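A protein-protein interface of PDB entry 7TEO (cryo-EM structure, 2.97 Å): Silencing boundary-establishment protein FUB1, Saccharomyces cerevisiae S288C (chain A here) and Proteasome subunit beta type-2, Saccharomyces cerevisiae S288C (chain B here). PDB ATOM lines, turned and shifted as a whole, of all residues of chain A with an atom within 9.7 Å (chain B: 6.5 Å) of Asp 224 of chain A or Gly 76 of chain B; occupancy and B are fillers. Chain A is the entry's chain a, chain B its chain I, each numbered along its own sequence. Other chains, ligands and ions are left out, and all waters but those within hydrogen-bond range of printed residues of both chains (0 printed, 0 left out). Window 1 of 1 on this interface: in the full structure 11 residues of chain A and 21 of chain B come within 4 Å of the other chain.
The side-chain hydroxyl (OG1) of Thr 30 of chain B is in hydrogen-bond range of the side-chain carboxylate (OD2) of Asp 224 of chain A, at 2.8 Å. The side-chain amino group (NZ) of Lys 222 of chain A lies within hydrogen-bond range of the side-chain hydroxyl (OG) of Ser 49 of chain B (3.5 Å). The backbone NH (N) of Gly 76 of chain B lies within hydrogen-bond range of the backbone carbonyl oxygen (O) of Asp 224 of chain A. The side-chain hydroxyl of Thr 77 of chain B is in hydrogen-bond range of the backbone carbonyl oxygen of Gly 216 of chain A. The backbone NH (N) of Ala 78 of chain B lies within hydrogen-bond range of the backbone carbonyl oxygen (O) of Lys 222 of chain A, 3.1 Å away. The backbone NH (N) of Gly 157 of chain B lies within hydrogen-bond range of the backbone carbonyl oxygen (O) of Pro 226 of chain A, 2.6 Å away. The backbone NH of Ser 158 of chain B lies within hydrogen-bond range of the backbone carbonyl oxygen of Glu 225 of chain A (3.1 Å).
N of Ser 158 of chain B lies within hydrogen-bond range of O of Thr 30 of chain B, at 3.0 Å. The backbone carbonyl oxygen (O) of Gly 197 of chain B is in hydrogen-bond range of the backbone NH (N) of Thr 30 of chain B (2.7 Å). The backbone carbonyl oxygen (O) of Tyr 126 of chain B sits at hydrogen-bond distance from the backbone NH (N) of Ala 75 of chain B. The backbone NH (N) of Thr 77 of chain B is in hydrogen-bond range of the backbone carbonyl oxygen (O) of Gly 124 of chain B (3.2 Å). OG1 of Thr 81 of chain B is in hydrogen-bond range of O of Ala 78 of chain B (2.5 Å). O of Ala 135 of chain A sits at hydrogen-bond distance from NH1 of Arg 138 of chain A, 2.9 Å away.
Ala 135 of chain A touches Tyr 126 of chain B (CA to OH, 3.4 Å). Gly 216 of chain A touches Asp 80 of chain B. Gly 124 of chain B touches Gly 216 of chain A. CG of Lys 222 of chain A touches O of Thr 50 of chain B, at 3.6 Å. Gly 76 of chain B touches Lys 222 of chain A (O to O, 3.9 Å). Thr 77 of chain B touches Lys 222 of chain A. OG1 of Thr 77 of chain B touches CD1 of Tyr 223 of chain A, at 3.3 Å. Asp 224 of chain A touches Ala 75 of chain B (O to C, 3.9 Å). Pro 226 of chain A touches Tyr 126 of chain B (CB to CD2, 3.5 Å). Gly 157 of chain B touches Phe 227 of chain A (O to CA, 3.6 Å).
Of the printed residues of chain B, Gly 216 of chain A touches Thr 77 (2.7 Å), Asp 80 (3.96 Å) and Gly 124 (3.9 Å). Asp 224 of chain A touches just these residues of chain B: Thr 30, Ala 75 and Gly 76. Of the printed residues of chain B, Glu 225 of chain A touches Gly 157 (3.3 Å) and Ser 158 (3.1 Å). Printed residues of chain A within 4 Å of Thr 30 of chain B: Asp 224 (2.8 Å). Of the printed residues of chain A, Ala 75 of chain B touches Asp 224. Of chain A, only Gly 216 (2.7 Å), Lys 222 (3.7 Å) and Tyr 223 (3.3 Å) come within 4 Å of Thr 77 of chain B. Ala 79 of chain B touches none of the printed residues of chain A. Of the printed residues of chain A, Leu 156 of chain B touches Pro 226 (3.6 Å). The nearest residue of chain B that does not touch Asp 224 of chain A is Thr 50 of chain B (4.3 Å). The nearest residue of chain A that does not touch Gly 76 of chain B is Pro 226 of chain A (4.6 Å). The nearest printed residue of chain A that does not touch Leu 156 of chain B is Phe 227 of chain A (4.3 Å).
Printed residues of chain A that touch a printed residue of chain B: Ala 135, Gly 216, Lys 222, Tyr 223, Asp 224, Glu 225, Pro 226 and Phe 227. Hydrophobic or aromatic side chains of chain A within 4 Å of the printed part of chain B: Ala 135, Tyr 223 and Pro 226. Printed residues of chain B that touch a printed residue of chain A: Thr 30, Ser 49, Thr 50, Ala 75, Gly 76, Thr 77, Ala 78, Asp 80, Gly 124, Tyr 126, Leu 156, Gly 157 and Ser 158. Hydrophobic or aromatic side chains of chain B that line the printed part of chain A: Ala 78, Tyr 126 and Leu 156. Among the printed residues, no Asp or Glu carboxylate lies within 4 Å of a Lys or Arg side-chain nitrogen of the other chain.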
ATOM      1  N   ALA A 135      31.102 -16.890 -15.330  1.00  0.00           N
ATOM      2  CA  ALA A 135      29.685 -17.216 -15.226  1.00  0.00           C
ATOM      3  C   ALA A 135      29.070 -16.690 -13.939  1.00  0.00           C
ATOM      4  O   ALA A 135      27.874 -16.381 -13.917  1.00  0.00           O
ATOM      5  CB  ALA A 135      29.486 -18.730 -15.311  1.00  0.00           C
ATOM      6  N   ARG A 138      29.004 -10.689 -11.751  1.00  0.00           N
ATOM      7  CA  ARG A 138      27.816  -9.899 -11.466  1.00  0.00           C
ATOM      8  C   ARG A 138      28.175  -8.425 -11.569  1.00  0.00           C
ATOM      9  O   ARG A 138      29.278  -8.021 -11.195  1.00  0.00           O
ATOM     10  CB  ARG A 138      27.262 -10.206 -10.069  1.00  0.00           C
ATOM     11  CG  ARG A 138      26.913 -11.670  -9.829  1.00  0.00           C
ATOM     12  CD  ARG A 138      25.745 -12.131 -10.689  1.00  0.00           C
ATOM     13  NE  ARG A 138      25.409 -13.529 -10.440  1.00  0.00           N
ATOM     14  CZ  ARG A 138      25.759 -14.548 -11.215  1.00  0.00           C
ATOM     15  NH1 ARG A 138      26.469 -14.372 -12.318  1.00  0.00           N
ATOM     16  NH2 ARG A 138      25.388 -15.778 -10.873  1.00  0.00           N
ATOM     17  N   MET A 213      22.787  -8.678 -10.373  1.00  0.00           N
ATOM     18  CA  MET A 213      22.432  -9.625 -11.416  1.00  0.00           C
ATOM     19  C   MET A 213      23.468  -9.606 -12.532  1.00  0.00           C
ATOM     20  O   MET A 213      24.187  -8.615 -12.709  1.00  0.00           O
ATOM     21  CB  MET A 213      21.046  -9.302 -11.990  1.00  0.00           C
ATOM     22  CG  MET A 213      19.900  -9.639 -11.052  1.00  0.00           C
ATOM     23  SD  MET A 213      19.708 -11.412 -10.793  1.00  0.00           S
ATOM     24  CE  MET A 213      18.936 -11.900 -12.332  1.00  0.00           C
ATOM     25  N   PRO A 214      23.575 -10.686 -13.305  1.00  0.00           N
ATOM     26  CA  PRO A 214      24.596 -10.732 -14.347  1.00  0.00           C
ATOM     27  C   PRO A 214      24.343  -9.684 -15.398  1.00  0.00           C
ATOM     28  O   PRO A 214      23.189  -9.267 -15.631  1.00  0.00           O
ATOM     29  CB  PRO A 214      24.453 -12.154 -14.912  1.00  0.00           C
ATOM     30  CG  PRO A 214      23.056 -12.539 -14.611  1.00  0.00           C
ATOM     31  CD  PRO A 214      22.751 -11.906 -13.289  1.00  0.00           C
ATOM     32  N   GLY A 216      24.120  -9.720 -18.553  1.00  0.00           N
ATOM     33  CA  GLY A 216      23.220 -10.085 -19.631  1.00  0.00           C
ATOM     34  C   GLY A 216      21.755 -10.044 -19.253  1.00  0.00           C
ATOM     35  O   GLY A 216      20.897 -10.155 -20.135  1.00  0.00           O
ATOM     36  N   TRP A 217      21.449  -9.896 -17.968  1.00  0.00           N
ATOM     37  CA  TRP A 217      20.068  -9.883 -17.511  1.00  0.00           C
ATOM     38  C   TRP A 217      19.406  -8.548 -17.825  1.00  0.00           C
ATOM     39  O   TRP A 217      19.994  -7.481 -17.627  1.00  0.00           O
ATOM     40  CB  TRP A 217      20.008 -10.154 -16.007  1.00  0.00           C
ATOM     41  CG  TRP A 217      18.618 -10.224 -15.457  1.00  0.00           C
ATOM     42  CD1 TRP A 217      17.685 -11.186 -15.707  1.00  0.00           C
ATOM     43  CD2 TRP A 217      18.007  -9.300 -14.549  1.00  0.00           C
ATOM     44  NE1 TRP A 217      16.529 -10.917 -15.016  1.00  0.00           N
ATOM     45  CE2 TRP A 217      16.702  -9.763 -14.297  1.00  0.00           C
ATOM     46  CE3 TRP A 217      18.437  -8.124 -13.927  1.00  0.00           C
ATOM     47  CZ2 TRP A 217      15.823  -9.094 -13.450  1.00  0.00           C
ATOM     48  CZ3 TRP A 217      17.562  -7.461 -13.089  1.00  0.00           C
ATOM     49  CH2 TRP A 217      16.270  -7.946 -12.858  1.00  0.00           C
ATOM     50  N   MET A 218      18.175  -8.618 -18.324  1.00  0.00           N
ATOM     51  CA  MET A 218      17.347  -7.456 -18.587  1.00  0.00           C
ATOM     52  C   MET A 218      16.117  -7.518 -17.691  1.00  0.00           C
ATOM     53  O   MET A 218      15.365  -8.501 -17.760  1.00  0.00           O
ATOM     54  CB  MET A 218      16.920  -7.414 -20.066  1.00  0.00           C
ATOM     55  CG  MET A 218      15.925  -6.315 -20.410  1.00  0.00           C
ATOM     56  SD  MET A 218      16.553  -4.664 -20.051  1.00  0.00           S
ATOM     57  CE  MET A 218      17.847  -4.514 -21.279  1.00  0.00           C
ATOM     58  N   SER A 221      12.811  -9.671 -18.403  1.00  0.00           N
ATOM     59  CA  SER A 221      13.002 -10.574 -19.526  1.00  0.00           C
ATOM     60  C   SER A 221      13.083 -12.020 -19.042  1.00  0.00           C
ATOM     61  O   SER A 221      13.457 -12.301 -17.900  1.00  0.00           O
ATOM     62  CB  SER A 221      14.270 -10.209 -20.297  1.00  0.00           C
ATOM     63  OG  SER A 221      15.427 -10.445 -19.515  1.00  0.00           O
ATOM     64  N   LYS A 222      12.727 -12.944 -19.931  1.00  0.00           N
ATOM     65  CA  LYS A 222      12.801 -14.362 -19.603  1.00  0.00           C
ATOM     66  C   LYS A 222      14.262 -14.775 -19.486  1.00  0.00           C
ATOM     67  O   LYS A 222      15.013 -14.710 -20.463  1.00  0.00           O
ATOM     68  CB  LYS A 222      12.090 -15.200 -20.664  1.00  0.00           C
ATOM     69  CG  LYS A 222      11.836 -16.638 -20.232  1.00  0.00           C
ATOM     70  CD  LYS A 222      11.824 -17.614 -21.404  1.00  0.00           C
ATOM     71  CE  LYS A 222      10.755 -17.274 -22.432  1.00  0.00           C
ATOM     72  NZ  LYS A 222      10.888 -18.103 -23.666  1.00  0.00           N
ATOM     73  N   TYR A 223      14.665 -15.198 -18.290  1.00  0.00           N
ATOM     74  CA  TYR A 223      16.047 -15.549 -18.003  1.00  0.00           C
ATOM     75  C   TYR A 223      16.115 -16.927 -17.365  1.00  0.00           C
ATOM     76  O   TYR A 223      15.312 -17.257 -16.487  1.00  0.00           O
ATOM     77  CB  TYR A 223      16.697 -14.515 -17.081  1.00  0.00           C
ATOM     78  CG  TYR A 223      18.180 -14.714 -16.893  1.00  0.00           C
ATOM     79  CD1 TYR A 223      19.090 -14.194 -17.802  1.00  0.00           C
ATOM     80  CD2 TYR A 223      18.672 -15.413 -15.801  1.00  0.00           C
ATOM     81  CE1 TYR A 223      20.446 -14.372 -17.633  1.00  0.00           C
ATOM     82  CE2 TYR A 223      20.026 -15.594 -15.623  1.00  0.00           C
ATOM     83  CZ  TYR A 223      20.909 -15.072 -16.541  1.00  0.00           C
ATOM     84  OH  TYR A 223      22.260 -15.250 -16.370  1.00  0.00           O
ATOM     85  N   ASP A 224      17.082 -17.725 -17.810  1.00  0.00           N
ATOM     86  CA  ASP A 224      17.321 -19.064 -17.285  1.00  0.00           C
ATOM     87  C   ASP A 224      18.756 -19.128 -16.791  1.00  0.00           C
ATOM     88  O   ASP A 224      19.690 -18.881 -17.562  1.00  0.00           O
ATOM     89  CB  ASP A 224      17.074 -20.125 -18.358  1.00  0.00           C
ATOM     90  CG  ASP A 224      15.612 -20.244 -18.736  1.00  0.00           C
ATOM     91  OD1 ASP A 224      14.746 -19.974 -17.878  1.00  0.00           O
ATOM     92  OD2 ASP A 224      15.329 -20.606 -19.897  1.00  0.00           O
ATOM     93  N   GLU A 225      18.936 -19.466 -15.521  1.00  0.00           N
ATOM     94  CA  GLU A 225      20.274 -19.485 -14.951  1.00  0.00           C
ATOM     95  C   GLU A 225      21.137 -20.488 -15.710  1.00  0.00           C
ATOM     96  O   GLU A 225      20.728 -21.645 -15.879  1.00  0.00           O
ATOM     97  CB  GLU A 225      20.229 -19.843 -13.466  1.00  0.00           C
ATOM     98  CG  GLU A 225      19.514 -18.818 -12.595  1.00  0.00           C
ATOM     99  CD  GLU A 225      18.004 -18.963 -12.625  1.00  0.00           C
ATOM    100  OE1 GLU A 225      17.503 -19.868 -13.323  1.00  0.00           O
ATOM    101  OE2 GLU A 225      17.317 -18.169 -11.946  1.00  0.00           O
ATOM    102  N   PRO A 226      22.323 -20.095 -16.185  1.00  0.00           N
ATOM    103  CA  PRO A 226      23.128 -21.035 -16.981  1.00  0.00           C
ATOM    104  C   PRO A 226      23.522 -22.284 -16.218  1.00  0.00           C
ATOM    105  O   PRO A 226      23.601 -23.361 -16.821  1.00  0.00           O
ATOM    106  CB  PRO A 226      24.350 -20.197 -17.374  1.00  0.00           C
ATOM    107  CG  PRO A 226      24.465 -19.182 -16.295  1.00  0.00           C
ATOM    108  CD  PRO A 226      23.054 -18.844 -15.918  1.00  0.00           C
ATOM    109  N   PHE A 227      23.779 -22.176 -14.916  1.00  0.00           N
ATOM    110  CA  PHE A 227      24.082 -23.332 -14.083  1.00  0.00           C
ATOM    111  C   PHE A 227      23.244 -23.413 -12.818  1.00  0.00           C
ATOM    112  O   PHE A 227      23.175 -24.493 -12.220  1.00  0.00           O
ATOM    113  CB  PHE A 227      25.566 -23.336 -13.685  1.00  0.00           C
ATOM    114  CG  PHE A 227      26.504 -23.066 -14.828  1.00  0.00           C
ATOM    115  CD1 PHE A 227      27.012 -24.110 -15.585  1.00  0.00           C
ATOM    116  CD2 PHE A 227      26.882 -21.772 -15.143  1.00  0.00           C
ATOM    117  CE1 PHE A 227      27.874 -23.867 -16.636  1.00  0.00           C
ATOM    118  CE2 PHE A 227      27.745 -21.523 -16.195  1.00  0.00           C
ATOM    119  CZ  PHE A 227      28.243 -22.572 -16.941  1.00  0.00           C
ATOM    120  N   GLY A 228      22.607 -22.327 -12.394  1.00  0.00           N
ATOM    121  CA  GLY A 228      21.839 -22.322 -11.173  1.00  0.00           C
ATOM    122  C   GLY A 228      22.742 -22.262  -9.957  1.00  0.00           C
ATOM    123  O   GLY A 228      23.444 -21.272  -9.733  1.00  0.00           O
ATOM    124  N   PRO A 229      22.745 -23.325  -9.137  1.00  0.00           N
ATOM    125  CA  PRO A 229      23.625 -23.313  -7.964  1.00  0.00           C
ATOM    126  C   PRO A 229      25.103 -23.414  -8.333  1.00  0.00           C
ATOM    127  O   PRO A 229      25.422 -23.912  -9.413  1.00  0.00           O
ATOM    128  CB  PRO A 229      23.175 -24.546  -7.177  1.00  0.00           C
ATOM    129  CG  PRO A 229      22.575 -25.444  -8.198  1.00  0.00           C
ATOM    130  CD  PRO A 229      21.911 -24.540  -9.181  1.00  0.00           C
ATOM    131  N   THR B  30      15.801 -24.769 -17.225  1.00  0.00           N
ATOM    132  CA  THR B  30      16.319 -25.409 -18.466  1.00  0.00           C
ATOM    133  C   THR B  30      17.283 -26.537 -18.138  1.00  0.00           C
ATOM    134  O   THR B  30      18.156 -26.390 -17.286  1.00  0.00           O
ATOM    135  CB  THR B  30      17.035 -24.391 -19.369  1.00  0.00           C
ATOM    136  OG1 THR B  30      16.198 -23.246 -19.565  1.00  0.00           O
ATOM    137  CG2 THR B  30      17.378 -25.010 -20.714  1.00  0.00           C
ATOM    138  N   ARG B  48       9.856 -27.312 -20.805  1.00  0.00           N
ATOM    139  CA  ARG B  48       9.193 -26.311 -19.980  1.00  0.00           C
ATOM    140  C   ARG B  48       9.869 -24.955 -20.145  1.00  0.00           C
ATOM    141  O   ARG B  48      11.098 -24.852 -20.155  1.00  0.00           O
ATOM    142  CB  ARG B  48       9.208 -26.726 -18.507  1.00  0.00           C
ATOM    143  CG  ARG B  48       8.715 -25.636 -17.562  1.00  0.00           C
ATOM    144  CD  ARG B  48       8.709 -26.068 -16.106  1.00  0.00           C
ATOM    145  NE  ARG B  48       7.668 -27.046 -15.813  1.00  0.00           N
ATOM    146  CZ  ARG B  48       7.619 -27.776 -14.709  1.00  0.00           C
ATOM    147  NH1 ARG B  48       8.528 -27.652 -13.755  1.00  0.00           N
ATOM    148  NH2 ARG B  48       6.630 -28.650 -14.552  1.00  0.00           N
ATOM    149  N   SER B  49       9.053 -23.911 -20.272  1.00  0.00           N
ATOM    150  CA  SER B  49       9.529 -22.535 -20.331  1.00  0.00           C
ATOM    151  C   SER B  49       8.831 -21.738 -19.242  1.00  0.00           C
ATOM    152  O   SER B  49       7.599 -21.740 -19.164  1.00  0.00           O
ATOM    153  CB  SER B  49       9.258 -21.914 -21.704  1.00  0.00           C
ATOM    154  OG  SER B  49       9.392 -20.505 -21.663  1.00  0.00           O
ATOM    155  N   THR B  50       9.612 -21.050 -18.414  1.00  0.00           N
ATOM    156  CA  THR B  50       9.099 -20.376 -17.230  1.00  0.00           C
ATOM    157  C   THR B  50       9.505 -18.911 -17.243  1.00  0.00           C
ATOM    158  O   THR B  50      10.672 -18.590 -17.485  1.00  0.00           O
ATOM    159  CB  THR B  50       9.620 -21.032 -15.947  1.00  0.00           C
ATOM    160  OG1 THR B  50      11.051 -20.971 -15.923  1.00  0.00           O
ATOM    161  CG2 THR B  50       9.188 -22.482 -15.871  1.00  0.00           C
ATOM    162  N   LYS B  62      13.488 -26.109 -27.541  1.00  0.00           N
ATOM    163  CA  LYS B  62      14.722 -25.428 -27.174  1.00  0.00           C
ATOM    164  C   LYS B  62      15.894 -25.742 -28.095  1.00  0.00           C
ATOM    165  O   LYS B  62      16.890 -25.011 -28.066  1.00  0.00           O
ATOM    166  CB  LYS B  62      15.098 -25.784 -25.735  1.00  0.00           C
ATOM    167  CG  LYS B  62      14.106 -25.256 -24.718  1.00  0.00           C
ATOM    168  CD  LYS B  62      14.494 -25.619 -23.303  1.00  0.00           C
ATOM    169  CE  LYS B  62      13.454 -25.127 -22.318  1.00  0.00           C
ATOM    170  NZ  LYS B  62      13.755 -25.562 -20.931  1.00  0.00           N
ATOM    171  N   GLY B  74      20.277 -23.225 -25.759  1.00  0.00           N
ATOM    172  CA  GLY B  74      20.848 -22.165 -24.955  1.00  0.00           C
ATOM    173  C   GLY B  74      20.162 -21.908 -23.633  1.00  0.00           C
ATOM    174  O   GLY B  74      19.033 -22.348 -23.401  1.00  0.00           O
ATOM    175  N   ALA B  75      20.857 -21.188 -22.753  1.00  0.00           N
ATOM    176  CA  ALA B  75      20.333 -20.770 -21.461  1.00  0.00           C
ATOM    177  C   ALA B  75      20.582 -19.275 -21.313  1.00  0.00           C
ATOM    178  O   ALA B  75      20.967 -18.593 -22.268  1.00  0.00           O
ATOM    179  CB  ALA B  75      20.974 -21.564 -20.318  1.00  0.00           C
ATOM    180  N   GLY B  76      20.358 -18.757 -20.110  1.00  0.00           N
ATOM    181  CA  GLY B  76      20.515 -17.332 -19.889  1.00  0.00           C
ATOM    182  C   GLY B  76      19.336 -16.550 -20.448  1.00  0.00           C
ATOM    183  O   GLY B  76      18.193 -17.008 -20.434  1.00  0.00           O
ATOM    184  N   THR B  77      19.625 -15.355 -20.952  1.00  0.00           N
ATOM    185  CA  THR B  77      18.585 -14.511 -21.531  1.00  0.00           C
ATOM    186  C   THR B  77      18.069 -15.170 -22.803  1.00  0.00           C
ATOM    187  O   THR B  77      18.787 -15.253 -23.802  1.00  0.00           O
ATOM    188  CB  THR B  77      19.129 -13.116 -21.821  1.00  0.00           C
ATOM    189  OG1 THR B  77      19.729 -12.579 -20.636  1.00  0.00           O
ATOM    190  CG2 THR B  77      18.006 -12.196 -22.267  1.00  0.00           C
ATOM    191  N   ALA B  78      16.816 -15.629 -22.768  1.00  0.00           N
ATOM    192  CA  ALA B  78      16.283 -16.427 -23.868  1.00  0.00           C
ATOM    193  C   ALA B  78      16.285 -15.643 -25.174  1.00  0.00           C
ATOM    194  O   ALA B  78      16.658 -16.170 -26.231  1.00  0.00           O
ATOM    195  CB  ALA B  78      14.869 -16.896 -23.530  1.00  0.00           C
ATOM    196  N   ALA B  79      15.865 -14.378 -25.121  1.00  0.00           N
ATOM    197  CA  ALA B  79      15.796 -13.571 -26.331  1.00  0.00           C
ATOM    198  C   ALA B  79      17.166 -13.444 -26.983  1.00  0.00           C
ATOM    199  O   ALA B  79      17.293 -13.512 -28.210  1.00  0.00           O
ATOM    200  CB  ALA B  79      15.228 -12.193 -26.005  1.00  0.00           C
ATOM    201  N   ASP B  80      18.206 -13.237 -26.174  1.00  0.00           N
ATOM    202  CA  ASP B  80      19.551 -13.132 -26.725  1.00  0.00           C
ATOM    203  C   ASP B  80      19.991 -14.437 -27.369  1.00  0.00           C
ATOM    204  O   ASP B  80      20.619 -14.424 -28.432  1.00  0.00           O
ATOM    205  CB  ASP B  80      20.542 -12.724 -25.642  1.00  0.00           C
ATOM    206  CG  ASP B  80      20.290 -11.333 -25.120  1.00  0.00           C
ATOM    207  OD1 ASP B  80      20.245 -10.393 -25.941  1.00  0.00           O
ATOM    208  OD2 ASP B  80      20.149 -11.170 -23.892  1.00  0.00           O
ATOM    209  N   THR B  81      19.693 -15.573 -26.739  1.00  0.00           N
ATOM    210  CA  THR B  81      20.034 -16.846 -27.360  1.00  0.00           C
ATOM    211  C   THR B  81      19.347 -16.992 -28.707  1.00  0.00           C
ATOM    212  O   THR B  81      19.982 -17.391 -29.690  1.00  0.00           O
ATOM    213  CB  THR B  81      19.653 -18.015 -26.449  1.00  0.00           C
ATOM    214  OG1 THR B  81      18.229 -18.063 -26.295  1.00  0.00           O
ATOM    215  CG2 THR B  81      20.308 -17.882 -25.082  1.00  0.00           C
ATOM    216  N   GLY B 124      24.612 -12.190 -22.794  1.00  0.00           N
ATOM    217  CA  GLY B 124      24.145 -13.147 -21.809  1.00  0.00           C
ATOM    218  C   GLY B 124      23.632 -14.460 -22.363  1.00  0.00           C
ATOM    219  O   GLY B 124      22.706 -15.047 -21.798  1.00  0.00           O
ATOM    220  N   ALA B 125      24.206 -14.931 -23.464  1.00  0.00           N
ATOM    221  CA  ALA B 125      23.791 -16.179 -24.089  1.00  0.00           C
ATOM    222  C   ALA B 125      24.769 -17.288 -23.715  1.00  0.00           C
ATOM    223  O   ALA B 125      25.966 -17.185 -23.997  1.00  0.00           O
ATOM    224  CB  ALA B 125      23.713 -16.024 -25.606  1.00  0.00           C
ATOM    225  N   TYR B 126      24.253 -18.343 -23.089  1.00  0.00           N
ATOM    226  CA  TYR B 126      25.011 -19.552 -22.809  1.00  0.00           C
ATOM    227  C   TYR B 126      24.457 -20.678 -23.668  1.00  0.00           C
ATOM    228  O   TYR B 126      23.245 -20.902 -23.697  1.00  0.00           O
ATOM    229  CB  TYR B 126      24.926 -19.930 -21.329  1.00  0.00           C
ATOM    230  CG  TYR B 126      25.700 -19.001 -20.428  1.00  0.00           C
ATOM    231  CD1 TYR B 126      25.291 -17.689 -20.243  1.00  0.00           C
ATOM    232  CD2 TYR B 126      26.842 -19.429 -19.769  1.00  0.00           C
ATOM    233  CE1 TYR B 126      25.992 -16.833 -19.425  1.00  0.00           C
ATOM    234  CE2 TYR B 126      27.552 -18.577 -18.949  1.00  0.00           C
ATOM    235  CZ  TYR B 126      27.123 -17.279 -18.783  1.00  0.00           C
ATOM    236  OH  TYR B 126      27.824 -16.421 -17.968  1.00  0.00           O
ATOM    237  N   LEU B 156      23.769 -27.924 -19.183  1.00  0.00           N
ATOM    238  CA  LEU B 156      23.544 -26.489 -19.104  1.00  0.00           C
ATOM    239  C   LEU B 156      22.168 -26.232 -18.509  1.00  0.00           C
ATOM    240  O   LEU B 156      21.299 -27.106 -18.500  1.00  0.00           O
ATOM    241  CB  LEU B 156      23.666 -25.835 -20.485  1.00  0.00           C
ATOM    242  CG  LEU B 156      23.838 -24.319 -20.535  1.00  0.00           C
ATOM    243  CD1 LEU B 156      25.215 -23.925 -20.029  1.00  0.00           C
ATOM    244  CD2 LEU B 156      23.623 -23.815 -21.946  1.00  0.00           C
ATOM    245  N   GLY B 157      21.981 -25.013 -18.012  1.00  0.00           N
ATOM    246  CA  GLY B 157      20.707 -24.608 -17.461  1.00  0.00           C
ATOM    247  C   GLY B 157      20.589 -24.905 -15.979  1.00  0.00           C
ATOM    248  O   GLY B 157      21.472 -25.486 -15.348  1.00  0.00           O
ATOM    249  N   SER B 158      19.454 -24.488 -15.415  1.00  0.00           N
ATOM    250  CA  SER B 158      19.226 -24.658 -13.984  1.00  0.00           C
ATOM    251  C   SER B 158      19.314 -26.114 -13.556  1.00  0.00           C
ATOM    252  O   SER B 158      19.676 -26.392 -12.408  1.00  0.00           O
ATOM    253  CB  SER B 158      17.858 -24.090 -13.603  1.00  0.00           C
ATOM    254  OG  SER B 158      16.819 -24.772 -14.281  1.00  0.00           O
ATOM    255  N   GLY B 197      12.766 -25.512 -12.535  1.00  0.00           N
ATOM    256  CA  GLY B 197      12.787 -24.800 -13.797  1.00  0.00           C
ATOM    257  C   GLY B 197      12.970 -25.701 -15.001  1.00  0.00           C
ATOM    258  O   GLY B 197      13.439 -25.256 -16.050  1.00  0.00           O
